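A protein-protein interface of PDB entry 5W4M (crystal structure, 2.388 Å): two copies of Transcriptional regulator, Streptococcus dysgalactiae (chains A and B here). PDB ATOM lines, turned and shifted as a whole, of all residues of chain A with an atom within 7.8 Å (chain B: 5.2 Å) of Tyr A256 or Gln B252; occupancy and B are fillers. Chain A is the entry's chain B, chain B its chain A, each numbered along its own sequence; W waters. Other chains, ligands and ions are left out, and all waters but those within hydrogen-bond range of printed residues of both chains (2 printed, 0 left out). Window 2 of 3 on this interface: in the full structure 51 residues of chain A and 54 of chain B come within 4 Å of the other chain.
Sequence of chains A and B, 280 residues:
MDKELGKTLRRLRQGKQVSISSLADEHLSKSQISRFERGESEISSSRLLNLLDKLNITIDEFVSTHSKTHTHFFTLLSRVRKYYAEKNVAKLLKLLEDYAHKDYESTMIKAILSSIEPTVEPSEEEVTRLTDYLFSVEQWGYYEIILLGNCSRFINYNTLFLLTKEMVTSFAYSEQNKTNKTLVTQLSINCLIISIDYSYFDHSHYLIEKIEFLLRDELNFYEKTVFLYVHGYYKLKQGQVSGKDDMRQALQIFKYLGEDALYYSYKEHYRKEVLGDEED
OH of Tyr B256 lies within hydrogen-bond range of NE2 of Gln B252, at 3.1 Å.
The side-chain amide oxygen (OE1) of Gln A252 is in hydrogen-bond range of the side-chain hydroxyl (OH) of Tyr A256 (2.7 Å).
Gln A249 touches Tyr B256 (CD to CD1, 3.4 Å).
Ile A253 touches Tyr B256 (CD1 to CB, 3.9 Å).
Ile A253 touches Leu B257.
Tyr A256 touches Gln B249.
Tyr A256 touches Gln B252.
Ile B253 touches Leu A257.
Of the printed residues of chain B, Gln A249 touches Tyr B256.
Printed residues of chain B within 4 Å of Ile A253: Tyr B256 and Leu B257.
Tyr A256 touches two residues of chain B.
Printed residues of chain B within 4 Å of Leu A257: Ile B253 (3.6 Å).
Of the printed residues of chain A, Gln B249 touches Tyr A256 (3.5 Å).
Of the printed residues of chain A, Gln B252 touches Tyr A256.
Printed residues of chain A within 4 Å of Tyr B256: Gln A249 (3.4 Å) and Ile A253 (3.9 Å).
The nearest residue of chain B that does not touch Tyr A256 is Ile B253 (4.1 Å).
Of the 13 printed residues of chain A, 4 touch a printed residue of chain B.
Printed residues of chain A that touch a printed residue of chain B: Gln A249, Ile A253, Tyr A256 and Leu A257.
Hydrophobic or aromatic side chains of chain A within 4 Å of the printed part of chain B: Ile A253, Tyr A256 and Leu A257.
Among the printed residues, 6 pairs touch across the chains.
Gln A249 touches Tyr B256, and with the chains exchanged Tyr A256 touches Gln B249.
Ile A253 touches Tyr B256, but with the chains exchanged Tyr A256 does not touch Ile B253 (4.1 Å).
Ile A253 touches Leu B257, and with the chains exchanged Leu A257 touches Ile B253.
Tyr A256 touches Gln B252, but with the chains exchanged Gln A252 does not touch Tyr B256 (4.1 Å).
9 positions are printed for both chains.
Water W1 bridges OE1 of Gln B249 (2.4 Å) and O of Tyr A256 (2.6 Å).
Water W2 lies within hydrogen-bond range of the side-chain amide oxygen of Gln A249 and the backbone carbonyl oxygen of Tyr B256.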
ATOM      1  N   GLN A 249     -21.456  31.520  18.637  1.00  0.00           N
ATOM      2  CA  GLN A 249     -20.593  31.670  19.804  1.00  0.00           C
ATOM      3  C   GLN A 249     -21.341  31.335  21.088  1.00  0.00           C
ATOM      4  O   GLN A 249     -20.765  30.762  22.021  1.00  0.00           O
ATOM      5  CB  GLN A 249     -20.038  33.090  19.871  1.00  0.00           C
ATOM      6  CG  GLN A 249     -18.930  33.378  18.882  1.00  0.00           C
ATOM      7  CD  GLN A 249     -18.545  34.843  18.878  1.00  0.00           C
ATOM      8  OE1 GLN A 249     -19.161  35.659  19.565  1.00  0.00           O
ATOM      9  NE2 GLN A 249     -17.521  35.184  18.106  1.00  0.00           N
ATOM     10  N   ALA A 250     -22.625  31.691  21.160  1.00  0.00           N
ATOM     11  CA  ALA A 250     -23.415  31.326  22.330  1.00  0.00           C
ATOM     12  C   ALA A 250     -23.583  29.815  22.425  1.00  0.00           C
ATOM     13  O   ALA A 250     -23.546  29.249  23.526  1.00  0.00           O
ATOM     14  CB  ALA A 250     -24.773  32.024  22.290  1.00  0.00           C
ATOM     15  N   LEU A 251     -23.753  29.142  21.282  1.00  0.00           N
ATOM     16  CA  LEU A 251     -23.817  27.682  21.280  1.00  0.00           C
ATOM     17  C   LEU A 251     -22.515  27.074  21.782  1.00  0.00           C
ATOM     18  O   LEU A 251     -22.528  26.084  22.523  1.00  0.00           O
ATOM     19  CB  LEU A 251     -24.138  27.163  19.877  1.00  0.00           C
ATOM     20  CG  LEU A 251     -25.516  27.489  19.296  1.00  0.00           C
ATOM     21  CD1 LEU A 251     -25.716  26.774  17.966  1.00  0.00           C
ATOM     22  CD2 LEU A 251     -26.618  27.120  20.277  1.00  0.00           C
ATOM     23  N   GLN A 252     -21.377  27.655  21.389  1.00  0.00           N
ATOM     24  CA  GLN A 252     -20.092  27.149  21.861  1.00  0.00           C
ATOM     25  C   GLN A 252     -19.956  27.290  23.371  1.00  0.00           C
ATOM     26  O   GLN A 252     -19.366  26.419  24.022  1.00  0.00           O
ATOM     27  CB  GLN A 252     -18.944  27.871  21.153  1.00  0.00           C
ATOM     28  CG  GLN A 252     -18.740  27.440  19.709  1.00  0.00           C
ATOM     29  CD  GLN A 252     -18.088  26.071  19.600  1.00  0.00           C
ATOM     30  OE1 GLN A 252     -16.893  25.916  19.860  1.00  0.00           O
ATOM     31  NE2 GLN A 252     -18.876  25.070  19.221  1.00  0.00           N
ATOM     32  N   ILE A 253     -20.496  28.369  23.940  1.00  0.00           N
ATOM     33  CA  ILE A 253     -20.442  28.555  25.389  1.00  0.00           C
ATOM     34  C   ILE A 253     -21.227  27.458  26.095  1.00  0.00           C
ATOM     35  O   ILE A 253     -20.745  26.853  27.060  1.00  0.00           O
ATOM     36  CB  ILE A 253     -20.953  29.958  25.763  1.00  0.00           C
ATOM     37  CG1 ILE A 253     -20.018  31.025  25.181  1.00  0.00           C
ATOM     38  CG2 ILE A 253     -21.088  30.096  27.278  1.00  0.00           C
ATOM     39  CD1 ILE A 253     -20.414  32.441  25.517  1.00  0.00           C
ATOM     40  N   PHE A 254     -22.447  27.178  25.621  1.00  0.00           N
ATOM     41  CA  PHE A 254     -23.223  26.075  26.181  1.00  0.00           C
ATOM     42  C   PHE A 254     -22.460  24.760  26.085  1.00  0.00           C
ATOM     43  O   PHE A 254     -22.493  23.942  27.012  1.00  0.00           O
ATOM     44  CB  PHE A 254     -24.569  25.953  25.462  1.00  0.00           C
ATOM     45  CG  PHE A 254     -25.529  27.072  25.758  1.00  0.00           C
ATOM     46  CD1 PHE A 254     -25.617  27.617  27.028  1.00  0.00           C
ATOM     47  CD2 PHE A 254     -26.349  27.576  24.757  1.00  0.00           C
ATOM     48  CE1 PHE A 254     -26.505  28.647  27.297  1.00  0.00           C
ATOM     49  CE2 PHE A 254     -27.241  28.606  25.018  1.00  0.00           C
ATOM     50  CZ  PHE A 254     -27.318  29.143  26.289  1.00  0.00           C
ATOM     51  N   LYS A 255     -21.762  24.541  24.968  1.00  0.00           N
ATOM     52  CA  LYS A 255     -21.065  23.277  24.756  1.00  0.00           C
ATOM     53  C   LYS A 255     -19.848  23.159  25.666  1.00  0.00           C
ATOM     54  O   LYS A 255     -19.655  22.135  26.333  1.00  0.00           O
ATOM     55  CB  LYS A 255     -20.664  23.148  23.284  1.00  0.00           C
ATOM     56  CG  LYS A 255     -19.888  21.888  22.939  1.00  0.00           C
ATOM     57  CD  LYS A 255     -19.384  21.943  21.504  1.00  0.00           C
ATOM     58  CE  LYS A 255     -18.232  20.972  21.279  1.00  0.00           C
ATOM     59  NZ  LYS A 255     -17.413  21.337  20.085  1.00  0.00           N
ATOM     60  N   TYR A 256     -19.020  24.206  25.716  1.00  0.00           N
ATOM     61  CA  TYR A 256     -17.816  24.168  26.544  1.00  0.00           C
ATOM     62  C   TYR A 256     -18.149  23.901  28.008  1.00  0.00           C
ATOM     63  O   TYR A 256     -17.407  23.194  28.702  1.00  0.00           O
ATOM     64  CB  TYR A 256     -17.043  25.482  26.408  1.00  0.00           C
ATOM     65  CG  TYR A 256     -16.406  25.688  25.052  1.00  0.00           C
ATOM     66  CD1 TYR A 256     -16.281  24.636  24.152  1.00  0.00           C
ATOM     67  CD2 TYR A 256     -15.931  26.936  24.672  1.00  0.00           C
ATOM     68  CE1 TYR A 256     -15.699  24.825  22.913  1.00  0.00           C
ATOM     69  CE2 TYR A 256     -15.345  27.132  23.434  1.00  0.00           C
ATOM     70  CZ  TYR A 256     -15.231  26.075  22.560  1.00  0.00           C
ATOM     71  OH  TYR A 256     -14.649  26.271  21.326  1.00  0.00           O
ATOM     72  N   LEU A 257     -19.261  24.448  28.496  1.00  0.00           N
ATOM     73  CA  LEU A 257     -19.661  24.288  29.889  1.00  0.00           C
ATOM     74  C   LEU A 257     -20.484  23.027  30.138  1.00  0.00           C
ATOM     75  O   LEU A 257     -20.986  22.840  31.251  1.00  0.00           O
ATOM     76  CB  LEU A 257     -20.447  25.516  30.357  1.00  0.00           C
ATOM     77  CG  LEU A 257     -19.702  26.846  30.257  1.00  0.00           C
ATOM     78  CD1 LEU A 257     -20.589  27.988  30.716  1.00  0.00           C
ATOM     79  CD2 LEU A 257     -18.414  26.801  31.065  1.00  0.00           C
ATOM     80  N   GLY A 258     -20.638  22.162  29.137  1.00  0.00           N
ATOM     81  CA  GLY A 258     -21.379  20.931  29.332  1.00  0.00           C
ATOM     82  C   GLY A 258     -22.870  21.096  29.524  1.00  0.00           C
ATOM     83  O   GLY A 258     -23.530  20.168  29.995  1.00  0.00           O
ATOM     84  N   GLU A 259     -23.425  22.255  29.170  1.00  0.00           N
ATOM     85  CA  GLU A 259     -24.863  22.501  29.288  1.00  0.00           C
ATOM     86  C   GLU A 259     -25.557  21.903  28.068  1.00  0.00           C
ATOM     87  O   GLU A 259     -25.939  22.595  27.121  1.00  0.00           O
ATOM     88  CB  GLU A 259     -25.141  23.992  29.424  1.00  0.00           C
ATOM     89  CG  GLU A 259     -24.537  24.611  30.671  1.00  0.00           C
ATOM     90  CD  GLU A 259     -25.237  24.155  31.934  1.00  0.00           C
ATOM     91  OE1 GLU A 259     -26.431  23.796  31.858  1.00  0.00           O
ATOM     92  OE2 GLU A 259     -24.593  24.150  33.003  1.00  0.00           O
ATOM     93  N   ASP A 260     -25.735  20.579  28.110  1.00  0.00           N
ATOM     94  CA  ASP A 260     -26.209  19.852  26.936  1.00  0.00           C
ATOM     95  C   ASP A 260     -27.654  20.199  26.599  1.00  0.00           C
ATOM     96  O   ASP A 260     -27.999  20.355  25.423  1.00  0.00           O
ATOM     97  CB  ASP A 260     -26.060  18.347  27.157  1.00  0.00           C
ATOM     98  CG  ASP A 260     -24.618  17.926  27.359  1.00  0.00           C
ATOM     99  OD1 ASP A 260     -23.709  18.747  27.108  1.00  0.00           O
ATOM    100  OD2 ASP A 260     -24.392  16.769  27.768  1.00  0.00           O
ATOM    101  N   TYR A 263     -27.755  23.546  25.095  1.00  0.00           N
ATOM    102  CA  TYR A 263     -27.083  23.507  23.798  1.00  0.00           C
ATOM    103  C   TYR A 263     -28.025  23.021  22.704  1.00  0.00           C
ATOM    104  O   TYR A 263     -28.096  23.613  21.622  1.00  0.00           O
ATOM    105  CB  TYR A 263     -25.840  22.615  23.875  1.00  0.00           C
ATOM    106  CG  TYR A 263     -25.170  22.387  22.538  1.00  0.00           C
ATOM    107  CD1 TYR A 263     -25.388  21.217  21.817  1.00  0.00           C
ATOM    108  CD2 TYR A 263     -24.324  23.344  21.994  1.00  0.00           C
ATOM    109  CE1 TYR A 263     -24.778  21.007  20.592  1.00  0.00           C
ATOM    110  CE2 TYR A 263     -23.709  23.145  20.770  1.00  0.00           C
ATOM    111  CZ  TYR A 263     -23.939  21.977  20.073  1.00  0.00           C
ATOM    112  OH  TYR A 263     -23.327  21.780  18.855  1.00  0.00           O
ATOM    113  N   LEU B 228     -13.822  25.873  34.937  1.00  0.00           N
ATOM    114  CA  LEU B 228     -13.324  25.202  33.739  1.00  0.00           C
ATOM    115  C   LEU B 228     -11.852  25.522  33.502  1.00  0.00           C
ATOM    116  O   LEU B 228     -11.063  24.634  33.158  1.00  0.00           O
ATOM    117  CB  LEU B 228     -14.160  25.602  32.526  1.00  0.00           C
ATOM    118  CG  LEU B 228     -13.648  25.132  31.163  1.00  0.00           C
ATOM    119  CD1 LEU B 228     -13.804  23.622  31.020  1.00  0.00           C
ATOM    120  CD2 LEU B 228     -14.368  25.864  30.036  1.00  0.00           C
ATOM    121  N   MET B 247      -8.585  25.413  29.449  1.00  0.00           N
ATOM    122  CA  MET B 247      -8.197  26.789  29.732  1.00  0.00           C
ATOM    123  C   MET B 247      -8.464  27.694  28.533  1.00  0.00           C
ATOM    124  O   MET B 247      -8.985  28.803  28.693  1.00  0.00           O
ATOM    125  CB  MET B 247      -6.728  26.831  30.149  1.00  0.00           C
ATOM    126  CG  MET B 247      -6.464  26.088  31.456  1.00  0.00           C
ATOM    127  SD  MET B 247      -4.763  26.181  32.047  1.00  0.00           S
ATOM    128  CE  MET B 247      -3.941  25.131  30.868  1.00  0.00           C
ATOM    129  N   ARG B 248      -8.137  27.229  27.324  1.00  0.00           N
ATOM    130  CA  ARG B 248      -8.427  28.011  26.126  1.00  0.00           C
ATOM    131  C   ARG B 248      -9.926  28.170  25.902  1.00  0.00           C
ATOM    132  O   ARG B 248     -10.370  29.219  25.423  1.00  0.00           O
ATOM    133  CB  ARG B 248      -7.779  27.367  24.897  1.00  0.00           C
ATOM    134  CG  ARG B 248      -6.269  27.217  24.989  1.00  0.00           C
ATOM    135  CD  ARG B 248      -5.636  27.083  23.609  1.00  0.00           C
ATOM    136  NE  ARG B 248      -4.410  26.289  23.647  1.00  0.00           N
ATOM    137  CZ  ARG B 248      -4.319  25.029  23.227  1.00  0.00           C
ATOM    138  NH1 ARG B 248      -5.381  24.412  22.728  1.00  0.00           N
ATOM    139  NH2 ARG B 248      -3.162  24.386  23.303  1.00  0.00           N
ATOM    140  N   GLN B 249     -10.719  27.145  26.225  1.00  0.00           N
ATOM    141  CA  GLN B 249     -12.167  27.274  26.105  1.00  0.00           C
ATOM    142  C   GLN B 249     -12.701  28.346  27.045  1.00  0.00           C
ATOM    143  O   GLN B 249     -13.563  29.146  26.662  1.00  0.00           O
ATOM    144  CB  GLN B 249     -12.839  25.932  26.388  1.00  0.00           C
ATOM    145  CG  GLN B 249     -12.698  24.929  25.262  1.00  0.00           C
ATOM    146  CD  GLN B 249     -13.264  23.568  25.617  1.00  0.00           C
ATOM    147  OE1 GLN B 249     -13.654  23.320  26.761  1.00  0.00           O
ATOM    148  NE2 GLN B 249     -13.313  22.675  24.635  1.00  0.00           N
ATOM    149  N   ALA B 250     -12.192  28.382  28.280  1.00  0.00           N
ATOM    150  CA  ALA B 250     -12.606  29.419  29.220  1.00  0.00           C
ATOM    151  C   ALA B 250     -12.234  30.805  28.707  1.00  0.00           C
ATOM    152  O   ALA B 250     -13.024  31.751  28.825  1.00  0.00           O
ATOM    153  CB  ALA B 250     -11.985  29.161  30.593  1.00  0.00           C
ATOM    154  N   LEU B 251     -11.036  30.945  28.130  1.00  0.00           N
ATOM    155  CA  LEU B 251     -10.659  32.214  27.512  1.00  0.00           C
ATOM    156  C   LEU B 251     -11.607  32.576  26.376  1.00  0.00           C
ATOM    157  O   LEU B 251     -11.969  33.745  26.207  1.00  0.00           O
ATOM    158  CB  LEU B 251      -9.218  32.148  27.005  1.00  0.00           C
ATOM    159  CG  LEU B 251      -8.120  31.974  28.057  1.00  0.00           C
ATOM    160  CD1 LEU B 251      -6.745  32.018  27.407  1.00  0.00           C
ATOM    161  CD2 LEU B 251      -8.237  33.031  29.144  1.00  0.00           C
ATOM    162  N   GLN B 252     -12.021  31.582  25.586  1.00  0.00           N
ATOM    163  CA  GLN B 252     -12.974  31.834  24.509  1.00  0.00           C
ATOM    164  C   GLN B 252     -14.294  32.365  25.053  1.00  0.00           C
ATOM    165  O   GLN B 252     -14.907  33.259  24.454  1.00  0.00           O
ATOM    166  CB  GLN B 252     -13.205  30.553  23.709  1.00  0.00           C
ATOM    167  CG  GLN B 252     -12.070  30.181  22.779  1.00  0.00           C
ATOM    168  CD  GLN B 252     -12.383  30.499  21.332  1.00  0.00           C
ATOM    169  OE1 GLN B 252     -12.314  31.654  20.906  1.00  0.00           O
ATOM    170  NE2 GLN B 252     -12.740  29.470  20.565  1.00  0.00           N
ATOM    171  N   ILE B 253     -14.747  31.825  26.186  1.00  0.00           N
ATOM    172  CA  ILE B 253     -15.999  32.284  26.778  1.00  0.00           C
ATOM    173  C   ILE B 253     -15.881  33.736  27.222  1.00  0.00           C
ATOM    174  O   ILE B 253     -16.784  34.546  26.974  1.00  0.00           O
ATOM    175  CB  ILE B 253     -16.412  31.363  27.939  1.00  0.00           C
ATOM    176  CG1 ILE B 253     -16.730  29.962  27.415  1.00  0.00           C
ATOM    177  CG2 ILE B 253     -17.610  31.939  28.678  1.00  0.00           C
ATOM    178  CD1 ILE B 253     -17.121  28.992  28.496  1.00  0.00           C
ATOM    179  N   PHE B 254     -14.773  34.088  27.885  1.00  0.00           N
ATOM    180  CA  PHE B 254     -14.547  35.480  28.272  1.00  0.00           C
ATOM    181  C   PHE B 254     -14.569  36.393  27.054  1.00  0.00           C
ATOM    182  O   PHE B 254     -15.244  37.429  27.051  1.00  0.00           O
ATOM    183  CB  PHE B 254     -13.215  35.619  29.013  1.00  0.00           C
ATOM    184  CG  PHE B 254     -13.204  34.993  30.379  1.00  0.00           C
ATOM    185  CD1 PHE B 254     -14.346  34.975  31.161  1.00  0.00           C
ATOM    186  CD2 PHE B 254     -12.047  34.417  30.879  1.00  0.00           C
ATOM    187  CE1 PHE B 254     -14.334  34.398  32.419  1.00  0.00           C
ATOM    188  CE2 PHE B 254     -12.027  33.839  32.132  1.00  0.00           C
ATOM    189  CZ  PHE B 254     -13.173  33.828  32.903  1.00  0.00           C
ATOM    190  N   LYS B 255     -13.845  36.012  26.000  1.00  0.00           N
ATOM    191  CA  LYS B 255     -13.815  36.824  24.787  1.00  0.00           C
ATOM    192  C   LYS B 255     -15.194  36.913  24.142  1.00  0.00           C
ATOM    193  O   LYS B 255     -15.625  38.000  23.740  1.00  0.00           O
ATOM    194  CB  LYS B 255     -12.794  36.254  23.802  1.00  0.00           C
ATOM    195  CG  LYS B 255     -12.707  37.006  22.484  1.00  0.00           C
ATOM    196  CD  LYS B 255     -12.024  36.171  21.406  1.00  0.00           C
ATOM    197  CE  LYS B 255     -10.582  35.857  21.771  1.00  0.00           C
ATOM    198  NZ  LYS B 255      -9.947  34.934  20.788  1.00  0.00           N
ATOM    199  N   TYR B 256     -15.904  35.784  24.042  1.00  0.00           N
ATOM    200  CA  TYR B 256     -17.215  35.787  23.396  1.00  0.00           C
ATOM    201  C   TYR B 256     -18.203  36.698  24.114  1.00  0.00           C
ATOM    202  O   TYR B 256     -19.061  37.310  23.468  1.00  0.00           O
ATOM    203  CB  TYR B 256     -17.778  34.366  23.323  1.00  0.00           C
ATOM    204  CG  TYR B 256     -17.108  33.480  22.301  1.00  0.00           C
ATOM    205  CD1 TYR B 256     -16.298  34.015  21.309  1.00  0.00           C
ATOM    206  CD2 TYR B 256     -17.286  32.103  22.330  1.00  0.00           C
ATOM    207  CE1 TYR B 256     -15.684  33.202  20.376  1.00  0.00           C
ATOM    208  CE2 TYR B 256     -16.678  31.284  21.404  1.00  0.00           C
ATOM    209  CZ  TYR B 256     -15.878  31.835  20.429  1.00  0.00           C
ATOM    210  OH  TYR B 256     -15.273  31.013  19.506  1.00  0.00           O
ATOM    211  N   LEU B 257     -18.103  36.801  25.436  1.00  0.00           N
ATOM    212  CA  LEU B 257     -19.006  37.633  26.218  1.00  0.00           C
ATOM    213  C   LEU B 257     -18.495  39.054  26.417  1.00  0.00           C
ATOM    214  O   LEU B 257     -19.135  39.831  27.136  1.00  0.00           O
ATOM    215  CB  LEU B 257     -19.267  36.993  27.582  1.00  0.00           C
ATOM    216  CG  LEU B 257     -19.924  35.617  27.538  1.00  0.00           C
ATOM    217  CD1 LEU B 257     -20.004  35.026  28.933  1.00  0.00           C
ATOM    218  CD2 LEU B 257     -21.307  35.736  26.914  1.00  0.00           C
HETATM  219  O   HOH W   1     -15.264  21.892  27.916  1.00  0.00           O
HETATM  220  O   HOH W   2     -18.863  38.010  20.717  1.00  0.00           O
